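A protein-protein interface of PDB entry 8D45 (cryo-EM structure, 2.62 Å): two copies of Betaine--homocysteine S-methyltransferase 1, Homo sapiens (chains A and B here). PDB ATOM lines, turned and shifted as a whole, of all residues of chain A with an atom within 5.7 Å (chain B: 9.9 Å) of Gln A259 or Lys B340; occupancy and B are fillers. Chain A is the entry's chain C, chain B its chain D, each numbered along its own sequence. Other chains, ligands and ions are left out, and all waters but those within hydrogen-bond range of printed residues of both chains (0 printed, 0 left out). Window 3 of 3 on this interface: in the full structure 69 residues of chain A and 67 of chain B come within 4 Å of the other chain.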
ATOM      1  N   GLU A 162      -5.946  28.991  37.640  1.00  0.00           N
ATOM      2  CA  GLU A 162      -4.802  28.944  36.739  1.00  0.00           C
ATOM      3  C   GLU A 162      -3.576  29.560  37.404  1.00  0.00           C
ATOM      4  O   GLU A 162      -2.569  28.881  37.626  1.00  0.00           O
ATOM      5  CB  GLU A 162      -5.137  29.658  35.430  1.00  0.00           C
ATOM      6  CG  GLU A 162      -6.121  28.891  34.562  1.00  0.00           C
ATOM      7  CD  GLU A 162      -6.348  29.536  33.210  1.00  0.00           C
ATOM      8  OE1 GLU A 162      -6.896  30.658  33.168  1.00  0.00           O
ATOM      9  OE2 GLU A 162      -5.987  28.917  32.187  1.00  0.00           O
ATOM     10  N   LEU A 193      -0.004  29.661  34.676  1.00  0.00           N
ATOM     11  CA  LEU A 193       0.075  30.625  33.583  1.00  0.00           C
ATOM     12  C   LEU A 193       1.265  31.561  33.744  1.00  0.00           C
ATOM     13  O   LEU A 193       1.940  31.874  32.757  1.00  0.00           O
ATOM     14  CB  LEU A 193      -1.223  31.433  33.497  1.00  0.00           C
ATOM     15  CG  LEU A 193      -2.409  30.882  32.694  1.00  0.00           C
ATOM     16  CD1 LEU A 193      -3.445  31.978  32.494  1.00  0.00           C
ATOM     17  CD2 LEU A 193      -1.994  30.307  31.342  1.00  0.00           C
ATOM     18  N   HIS A 218      -8.957  20.261  33.038  1.00  0.00           N
ATOM     19  CA  HIS A 218      -8.072  20.692  31.958  1.00  0.00           C
ATOM     20  C   HIS A 218      -7.164  19.598  31.412  1.00  0.00           C
ATOM     21  O   HIS A 218      -6.576  19.776  30.344  1.00  0.00           O
ATOM     22  CB  HIS A 218      -7.196  21.869  32.410  1.00  0.00           C
ATOM     23  CG  HIS A 218      -7.794  23.216  32.139  1.00  0.00           C
ATOM     24  ND1 HIS A 218      -7.059  24.380  32.217  1.00  0.00           N
ATOM     25  CD2 HIS A 218      -9.053  23.589  31.810  1.00  0.00           C
ATOM     26  CE1 HIS A 218      -7.836  25.410  31.934  1.00  0.00           C
ATOM     27  NE2 HIS A 218      -9.052  24.956  31.684  1.00  0.00           N
ATOM     28  N   PHE A 219      -7.072  18.451  32.079  1.00  0.00           N
ATOM     29  CA  PHE A 219      -6.207  17.381  31.600  1.00  0.00           C
ATOM     30  C   PHE A 219      -6.770  16.040  32.039  1.00  0.00           C
ATOM     31  O   PHE A 219      -7.502  15.940  33.023  1.00  0.00           O
ATOM     32  CB  PHE A 219      -4.753  17.511  32.093  1.00  0.00           C
ATOM     33  CG  PHE A 219      -4.141  18.869  31.875  1.00  0.00           C
ATOM     34  CD1 PHE A 219      -4.289  19.881  32.810  1.00  0.00           C
ATOM     35  CD2 PHE A 219      -3.431  19.138  30.720  1.00  0.00           C
ATOM     36  CE1 PHE A 219      -3.731  21.126  32.598  1.00  0.00           C
ATOM     37  CE2 PHE A 219      -2.875  20.379  30.504  1.00  0.00           C
ATOM     38  CZ  PHE A 219      -3.024  21.373  31.443  1.00  0.00           C
ATOM     39  N   ASN A 257      -2.114  21.085  24.580  1.00  0.00           N
ATOM     40  CA  ASN A 257      -0.994  21.947  24.911  1.00  0.00           C
ATOM     41  C   ASN A 257      -1.160  22.436  26.349  1.00  0.00           C
ATOM     42  O   ASN A 257      -1.959  21.901  27.122  1.00  0.00           O
ATOM     43  CB  ASN A 257      -0.883  23.100  23.907  1.00  0.00           C
ATOM     44  CG  ASN A 257      -2.092  24.018  23.915  1.00  0.00           C
ATOM     45  OD1 ASN A 257      -2.874  24.034  24.862  1.00  0.00           O
ATOM     46  ND2 ASN A 257      -2.236  24.807  22.860  1.00  0.00           N
ATOM     47  N   LYS A 258      -0.388  23.456  26.722  1.00  0.00           N
ATOM     48  CA  LYS A 258      -0.451  23.972  28.084  1.00  0.00           C
ATOM     49  C   LYS A 258      -1.855  24.432  28.460  1.00  0.00           C
ATOM     50  O   LYS A 258      -2.215  24.413  29.642  1.00  0.00           O
ATOM     51  CB  LYS A 258       0.539  25.128  28.250  1.00  0.00           C
ATOM     52  CG  LYS A 258       0.195  26.355  27.422  1.00  0.00           C
ATOM     53  CD  LYS A 258       1.395  26.899  26.661  1.00  0.00           C
ATOM     54  CE  LYS A 258       0.956  27.805  25.518  1.00  0.00           C
ATOM     55  NZ  LYS A 258       0.352  27.046  24.389  1.00  0.00           N
ATOM     56  N   GLN A 259      -2.663  24.840  27.482  1.00  0.00           N
ATOM     57  CA  GLN A 259      -3.994  25.384  27.754  1.00  0.00           C
ATOM     58  C   GLN A 259      -5.057  24.299  27.858  1.00  0.00           C
ATOM     59  O   GLN A 259      -6.121  24.414  27.247  1.00  0.00           O
ATOM     60  CB  GLN A 259      -4.372  26.394  26.675  1.00  0.00           C
ATOM     61  CG  GLN A 259      -3.304  27.439  26.354  1.00  0.00           C
ATOM     62  CD  GLN A 259      -3.200  28.532  27.404  1.00  0.00           C
ATOM     63  OE1 GLN A 259      -2.107  28.852  27.872  1.00  0.00           O
ATOM     64  NE2 GLN A 259      -4.334  29.118  27.771  1.00  0.00           N
ATOM     65  N   GLY A 260      -4.798  23.250  28.637  1.00  0.00           N
ATOM     66  CA  GLY A 260      -5.762  22.197  28.899  1.00  0.00           C
ATOM     67  C   GLY A 260      -6.551  21.707  27.702  1.00  0.00           C
ATOM     68  O   GLY A 260      -6.028  21.643  26.587  1.00  0.00           O
ATOM     69  N   PHE A 261      -7.822  21.359  27.929  1.00  0.00           N
ATOM     70  CA  PHE A 261      -8.687  20.885  26.853  1.00  0.00           C
ATOM     71  C   PHE A 261      -9.647  21.953  26.346  1.00  0.00           C
ATOM     72  O   PHE A 261     -10.463  21.659  25.469  1.00  0.00           O
ATOM     73  CB  PHE A 261      -9.469  19.642  27.303  1.00  0.00           C
ATOM     74  CG  PHE A 261     -10.702  19.935  28.125  1.00  0.00           C
ATOM     75  CD1 PHE A 261     -10.645  20.732  29.255  1.00  0.00           C
ATOM     76  CD2 PHE A 261     -11.925  19.394  27.764  1.00  0.00           C
ATOM     77  CE1 PHE A 261     -11.778  20.985  30.005  1.00  0.00           C
ATOM     78  CE2 PHE A 261     -13.061  19.647  28.509  1.00  0.00           C
ATOM     79  CZ  PHE A 261     -12.986  20.445  29.630  1.00  0.00           C
ATOM     80  N   ILE A 262      -9.566  23.181  26.862  1.00  0.00           N
ATOM     81  CA  ILE A 262     -10.382  24.262  26.316  1.00  0.00           C
ATOM     82  C   ILE A 262      -9.966  24.573  24.888  1.00  0.00           C
ATOM     83  O   ILE A 262     -10.805  24.929  24.052  1.00  0.00           O
ATOM     84  CB  ILE A 262     -10.287  25.522  27.201  1.00  0.00           C
ATOM     85  CG1 ILE A 262     -10.635  25.240  28.670  1.00  0.00           C
ATOM     86  CG2 ILE A 262     -11.213  26.615  26.671  1.00  0.00           C
ATOM     87  CD1 ILE A 262     -11.609  24.111  28.915  1.00  0.00           C
ATOM     88  N   ASP A 263      -8.673  24.467  24.584  1.00  0.00           N
ATOM     89  CA  ASP A 263      -8.158  24.863  23.283  1.00  0.00           C
ATOM     90  C   ASP A 263      -8.256  23.765  22.233  1.00  0.00           C
ATOM     91  O   ASP A 263      -7.992  24.034  21.056  1.00  0.00           O
ATOM     92  CB  ASP A 263      -6.703  25.314  23.415  1.00  0.00           C
ATOM     93  CG  ASP A 263      -6.581  26.703  24.001  1.00  0.00           C
ATOM     94  OD1 ASP A 263      -7.510  27.132  24.713  1.00  0.00           O
ATOM     95  OD2 ASP A 263      -5.553  27.366  23.757  1.00  0.00           O
ATOM     96  N   LEU A 264      -8.627  22.551  22.615  1.00  0.00           N
ATOM     97  CA  LEU A 264      -8.894  21.526  21.623  1.00  0.00           C
ATOM     98  C   LEU A 264     -10.055  21.973  20.737  1.00  0.00           C
ATOM     99  O   LEU A 264     -11.002  22.592  21.240  1.00  0.00           O
ATOM    100  CB  LEU A 264      -9.232  20.197  22.300  1.00  0.00           C
ATOM    101  CG  LEU A 264      -8.095  19.514  23.057  1.00  0.00           C
ATOM    102  CD1 LEU A 264      -8.591  18.254  23.724  1.00  0.00           C
ATOM    103  CD2 LEU A 264      -6.943  19.198  22.122  1.00  0.00           C
ATOM    104  N   GLY A 372      -5.739  26.977  20.112  1.00  0.00           N
ATOM    105  CA  GLY A 372      -4.982  28.061  20.706  1.00  0.00           C
ATOM    106  C   GLY A 372      -3.528  27.705  20.941  1.00  0.00           C
ATOM    107  O   GLY A 372      -2.723  28.563  21.306  1.00  0.00           O
ATOM    108  N   LEU B 335     -21.705  29.799  22.951  1.00  0.00           N
ATOM    109  CA  LEU B 335     -20.297  30.052  23.221  1.00  0.00           C
ATOM    110  C   LEU B 335     -19.831  31.400  22.691  1.00  0.00           C
ATOM    111  O   LEU B 335     -18.633  31.694  22.750  1.00  0.00           O
ATOM    112  CB  LEU B 335     -19.425  28.940  22.631  1.00  0.00           C
ATOM    113  CG  LEU B 335     -19.922  27.502  22.762  1.00  0.00           C
ATOM    114  CD1 LEU B 335     -19.113  26.589  21.859  1.00  0.00           C
ATOM    115  CD2 LEU B 335     -19.843  27.046  24.208  1.00  0.00           C
ATOM    116  N   ASP B 336     -20.743  32.229  22.178  1.00  0.00           N
ATOM    117  CA  ASP B 336     -20.351  33.576  21.777  1.00  0.00           C
ATOM    118  C   ASP B 336     -19.867  34.416  22.953  1.00  0.00           C
ATOM    119  O   ASP B 336     -19.221  35.446  22.735  1.00  0.00           O
ATOM    120  CB  ASP B 336     -21.520  34.284  21.095  1.00  0.00           C
ATOM    121  CG  ASP B 336     -22.483  34.905  22.088  1.00  0.00           C
ATOM    122  OD1 ASP B 336     -23.188  34.151  22.791  1.00  0.00           O
ATOM    123  OD2 ASP B 336     -22.530  36.151  22.171  1.00  0.00           O
ATOM    124  N   MET B 337     -20.165  34.002  24.187  1.00  0.00           N
ATOM    125  CA  MET B 337     -19.786  34.784  25.359  1.00  0.00           C
ATOM    126  C   MET B 337     -18.300  34.672  25.675  1.00  0.00           C
ATOM    127  O   MET B 337     -17.745  35.560  26.332  1.00  0.00           O
ATOM    128  CB  MET B 337     -20.610  34.331  26.565  1.00  0.00           C
ATOM    129  CG  MET B 337     -20.239  32.943  27.084  1.00  0.00           C
ATOM    130  SD  MET B 337     -18.885  32.929  28.280  1.00  0.00           S
ATOM    131  CE  MET B 337     -19.671  33.679  29.702  1.00  0.00           C
ATOM    132  N   HIS B 338     -17.645  33.599  25.230  1.00  0.00           N
ATOM    133  CA  HIS B 338     -16.311  33.253  25.715  1.00  0.00           C
ATOM    134  C   HIS B 338     -15.321  34.397  25.544  1.00  0.00           C
ATOM    135  O   HIS B 338     -15.549  35.318  24.753  1.00  0.00           O
ATOM    136  CB  HIS B 338     -15.785  32.009  24.995  1.00  0.00           C
ATOM    137  CG  HIS B 338     -15.027  31.076  25.887  1.00  0.00           C
ATOM    138  ND1 HIS B 338     -15.650  30.230  26.778  1.00  0.00           N
ATOM    139  CD2 HIS B 338     -13.697  30.873  26.042  1.00  0.00           C
ATOM    140  CE1 HIS B 338     -14.738  29.534  27.432  1.00  0.00           C
ATOM    141  NE2 HIS B 338     -13.545  29.906  27.006  1.00  0.00           N
ATOM    142  N   THR B 339     -14.218  34.343  26.287  1.00  0.00           N
ATOM    143  CA  THR B 339     -13.188  35.372  26.254  1.00  0.00           C
ATOM    144  C   THR B 339     -12.090  35.089  25.236  1.00  0.00           C
ATOM    145  O   THR B 339     -11.178  35.908  25.092  1.00  0.00           O
ATOM    146  CB  THR B 339     -12.562  35.528  27.646  1.00  0.00           C
ATOM    147  OG1 THR B 339     -11.913  36.801  27.744  1.00  0.00           O
ATOM    148  CG2 THR B 339     -11.552  34.417  27.916  1.00  0.00           C
ATOM    149  N   LYS B 340     -12.155  33.959  24.532  1.00  0.00           N
ATOM    150  CA  LYS B 340     -11.127  33.567  23.587  1.00  0.00           C
ATOM    151  C   LYS B 340     -11.695  33.528  22.174  1.00  0.00           C
ATOM    152  O   LYS B 340     -12.852  33.135  21.989  1.00  0.00           O
ATOM    153  CB  LYS B 340     -10.561  32.187  23.942  1.00  0.00           C
ATOM    154  CG  LYS B 340     -10.207  32.022  25.411  1.00  0.00           C
ATOM    155  CD  LYS B 340      -9.542  30.683  25.671  1.00  0.00           C
ATOM    156  CE  LYS B 340      -8.216  30.847  26.390  1.00  0.00           C
ATOM    157  NZ  LYS B 340      -7.565  29.535  26.648  1.00  0.00           N
ATOM    158  N   PRO B 341     -10.919  33.922  21.158  1.00  0.00           N
ATOM    159  CA  PRO B 341     -11.448  33.904  19.787  1.00  0.00           C
ATOM    160  C   PRO B 341     -11.576  32.513  19.193  1.00  0.00           C
ATOM    161  O   PRO B 341     -12.398  32.324  18.286  1.00  0.00           O
ATOM    162  CB  PRO B 341     -10.420  34.740  19.016  1.00  0.00           C
ATOM    163  CG  PRO B 341      -9.146  34.485  19.731  1.00  0.00           C
ATOM    164  CD  PRO B 341      -9.509  34.350  21.190  1.00  0.00           C
ATOM    165  N   TRP B 342     -10.800  31.541  19.669  1.00  0.00           N
ATOM    166  CA  TRP B 342     -10.884  30.182  19.152  1.00  0.00           C
ATOM    167  C   TRP B 342     -11.920  29.336  19.876  1.00  0.00           C
ATOM    168  O   TRP B 342     -12.135  28.182  19.490  1.00  0.00           O
ATOM    169  CB  TRP B 342      -9.518  29.495  19.233  1.00  0.00           C
ATOM    170  CG  TRP B 342      -8.944  29.418  20.611  1.00  0.00           C
ATOM    171  CD1 TRP B 342      -9.282  28.534  21.592  1.00  0.00           C
ATOM    172  CD2 TRP B 342      -7.934  30.267  21.165  1.00  0.00           C
ATOM    173  NE1 TRP B 342      -8.541  28.777  22.724  1.00  0.00           N
ATOM    174  CE2 TRP B 342      -7.706  29.837  22.486  1.00  0.00           C
ATOM    175  CE3 TRP B 342      -7.199  31.348  20.671  1.00  0.00           C
ATOM    176  CZ2 TRP B 342      -6.774  30.448  23.319  1.00  0.00           C
ATOM    177  CZ3 TRP B 342      -6.275  31.954  21.498  1.00  0.00           C
ATOM    178  CH2 TRP B 342      -6.070  31.504  22.808  1.00  0.00           C
ATOM    179  N   VAL B 343     -12.546  29.873  20.927  1.00  0.00           N
ATOM    180  CA  VAL B 343     -13.721  29.262  21.535  1.00  0.00           C
ATOM    181  C   VAL B 343     -14.975  30.092  21.306  1.00  0.00           C
ATOM    182  O   VAL B 343     -16.079  29.640  21.638  1.00  0.00           O
ATOM    183  CB  VAL B 343     -13.506  29.028  23.044  1.00  0.00           C
ATOM    184  CG1 VAL B 343     -14.483  27.984  23.570  1.00  0.00           C
ATOM    185  CG2 VAL B 343     -12.073  28.599  23.322  1.00  0.00           C
ATOM    186  N   ARG B 344     -14.838  31.291  20.743  1.00  0.00           N
ATOM    187  CA  ARG B 344     -15.966  32.125  20.350  1.00  0.00           C
ATOM    188  C   ARG B 344     -16.411  31.869  18.919  1.00  0.00           C
ATOM    189  O   ARG B 344     -17.613  31.856  18.642  1.00  0.00           O
ATOM    190  CB  ARG B 344     -15.603  33.604  20.500  1.00  0.00           C
ATOM    191  CG  ARG B 344     -16.008  34.230  21.822  1.00  0.00           C
ATOM    192  CD  ARG B 344     -16.139  35.735  21.677  1.00  0.00           C
ATOM    193  NE  ARG B 344     -15.007  36.297  20.950  1.00  0.00           N
ATOM    194  CZ  ARG B 344     -13.812  36.524  21.478  1.00  0.00           C
ATOM    195  NH1 ARG B 344     -13.550  36.247  22.746  1.00  0.00           N
ATOM    196  NH2 ARG B 344     -12.851  37.036  20.714  1.00  0.00           N
ATOM    197  N   ALA B 345     -15.465  31.671  18.001  1.00  0.00           N
ATOM    198  CA  ALA B 345     -15.790  31.327  16.625  1.00  0.00           C
ATOM    199  C   ALA B 345     -16.276  29.892  16.482  1.00  0.00           C
ATOM    200  O   ALA B 345     -16.754  29.520  15.405  1.00  0.00           O
ATOM    201  CB  ALA B 345     -14.573  31.553  15.725  1.00  0.00           C
ATOM    202  N   ARG B 346     -16.164  29.080  17.536  1.00  0.00           N
ATOM    203  CA  ARG B 346     -16.771  27.755  17.518  1.00  0.00           C
ATOM    204  C   ARG B 346     -18.290  27.844  17.526  1.00  0.00           C
ATOM    205  O   ARG B 346     -18.973  26.841  17.295  1.00  0.00           O
ATOM    206  CB  ARG B 346     -16.281  26.940  18.717  1.00  0.00           C
ATOM    207  CG  ARG B 346     -14.810  26.594  18.649  1.00  0.00           C
ATOM    208  CD  ARG B 346     -14.432  25.506  19.635  1.00  0.00           C
ATOM    209  NE  ARG B 346     -12.983  25.380  19.764  1.00  0.00           N
ATOM    210  CZ  ARG B 346     -12.337  25.104  20.889  1.00  0.00           C
ATOM    211  NH1 ARG B 346     -12.977  24.883  22.026  1.00  0.00           N
ATOM    212  NH2 ARG B 346     -11.009  25.037  20.874  1.00  0.00           N
ATOM    213  N   ALA B 347     -18.834  29.029  17.798  1.00  0.00           N
ATOM    214  CA  ALA B 347     -20.272  29.229  17.879  1.00  0.00           C
ATOM    215  C   ALA B 347     -20.886  29.528  16.516  1.00  0.00           C
ATOM    216  O   ALA B 347     -21.257  30.672  16.238  1.00  0.00           O
ATOM    217  CB  ALA B 347     -20.577  30.370  18.852  1.00  0.00           C
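No position is printed for both chains. Of the 8 pairs that touch across the chains among the printed residues, none has its exchanged pair printed and touching as well.
NE2 of Gln A259 lies close to NZ of Lys B340, at 3.4 Å. NH1 of Arg B346 lies within hydrogen-bond range of O of Ile A262 (3.0 Å). The side-chain carboxylate (OD1) of Asp A263 is in salt-bridge range of the side-chain amino group (NZ) of Lys B340, 3.1 Å away. OD1 of Asp A263 is in hydrogen-bond range of NE1 of Trp B342. The backbone carbonyl oxygen (O) of Asp A263 sits at hydrogen-bond distance from the guanidinium group (NH2) of Arg B346, at 3.2 Å. The backbone carbonyl oxygen (O) of Leu A264 lies within hydrogen-bond range of the guanidinium group (NH2) of Arg B346, at 2.5 Å.
Hydrophobic or aromatic side chains of chain A that line the printed part of chain B: Ile A262. Along chain A the printed residues that touch a printed residue of chain B span positions 259 to 372. Printed residues of chain B that touch a printed residue of chain A: Lys B340, Trp B342, Val B343 and Arg B346. Hydrophobic or aromatic side chains of chain B within 4 Å of the printed part of chain A: Trp B342 and Val B343. Among the printed residues, Asp or Glu carboxylates within 4 Å of a Lys or Arg side-chain nitrogen of the other chain: Asp A263 with Lys B340.
The backbone NH (N) of Gln A259 lies within hydrogen-bond range of the side-chain amide oxygen (OD1) of Asn A257 (2.7 Å). The guanidinium group of Arg B344 lies close to the backbone carbonyl oxygen of Lys B340 (3.3 Å). O of Trp B342 lies within hydrogen-bond range of NE of Arg B346 (2.9 Å).
Gln A259 touches just one residue of chain B: Lys B340 (3.4 Å). No residue of chain B comes within 4 Å of Lys A258. No residue of chain B comes within 4 Å of Gly A260. Printed residues of chain B within 4 Å of Ile A262: Val B343 and Arg B346. Printed residues of chain B within 4 Å of Asp A263: Lys B340, Trp B342 and Arg B346. Of the printed residues of chain A, Val B343 touches Ile A262. Of the printed residues of chain A, Arg B346 touches Ile A262 (3.0 Å), Asp A263 (3.2 Å) and Leu A264 (2.5 Å). Of the printed residues of chain B, Leu A264 touches Arg B346. Ala B345 touches none of the printed residues of chain A. Glu A162 touches none of the printed residues of chain B. The nearest residue of chain B that does not touch Gln A259 is Trp B342 (5.2 Å). The nearest residue of chain A that does not touch Lys B340 is Ile A262 (4.5 Å). The nearest printed residue of chain A that does not touch Trp B342 is Ile A262 (4.6 Å).
Among the printed residues, merely in contact across the chains: Ile A262 with Val B343 and Gly A372 with Trp B342.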
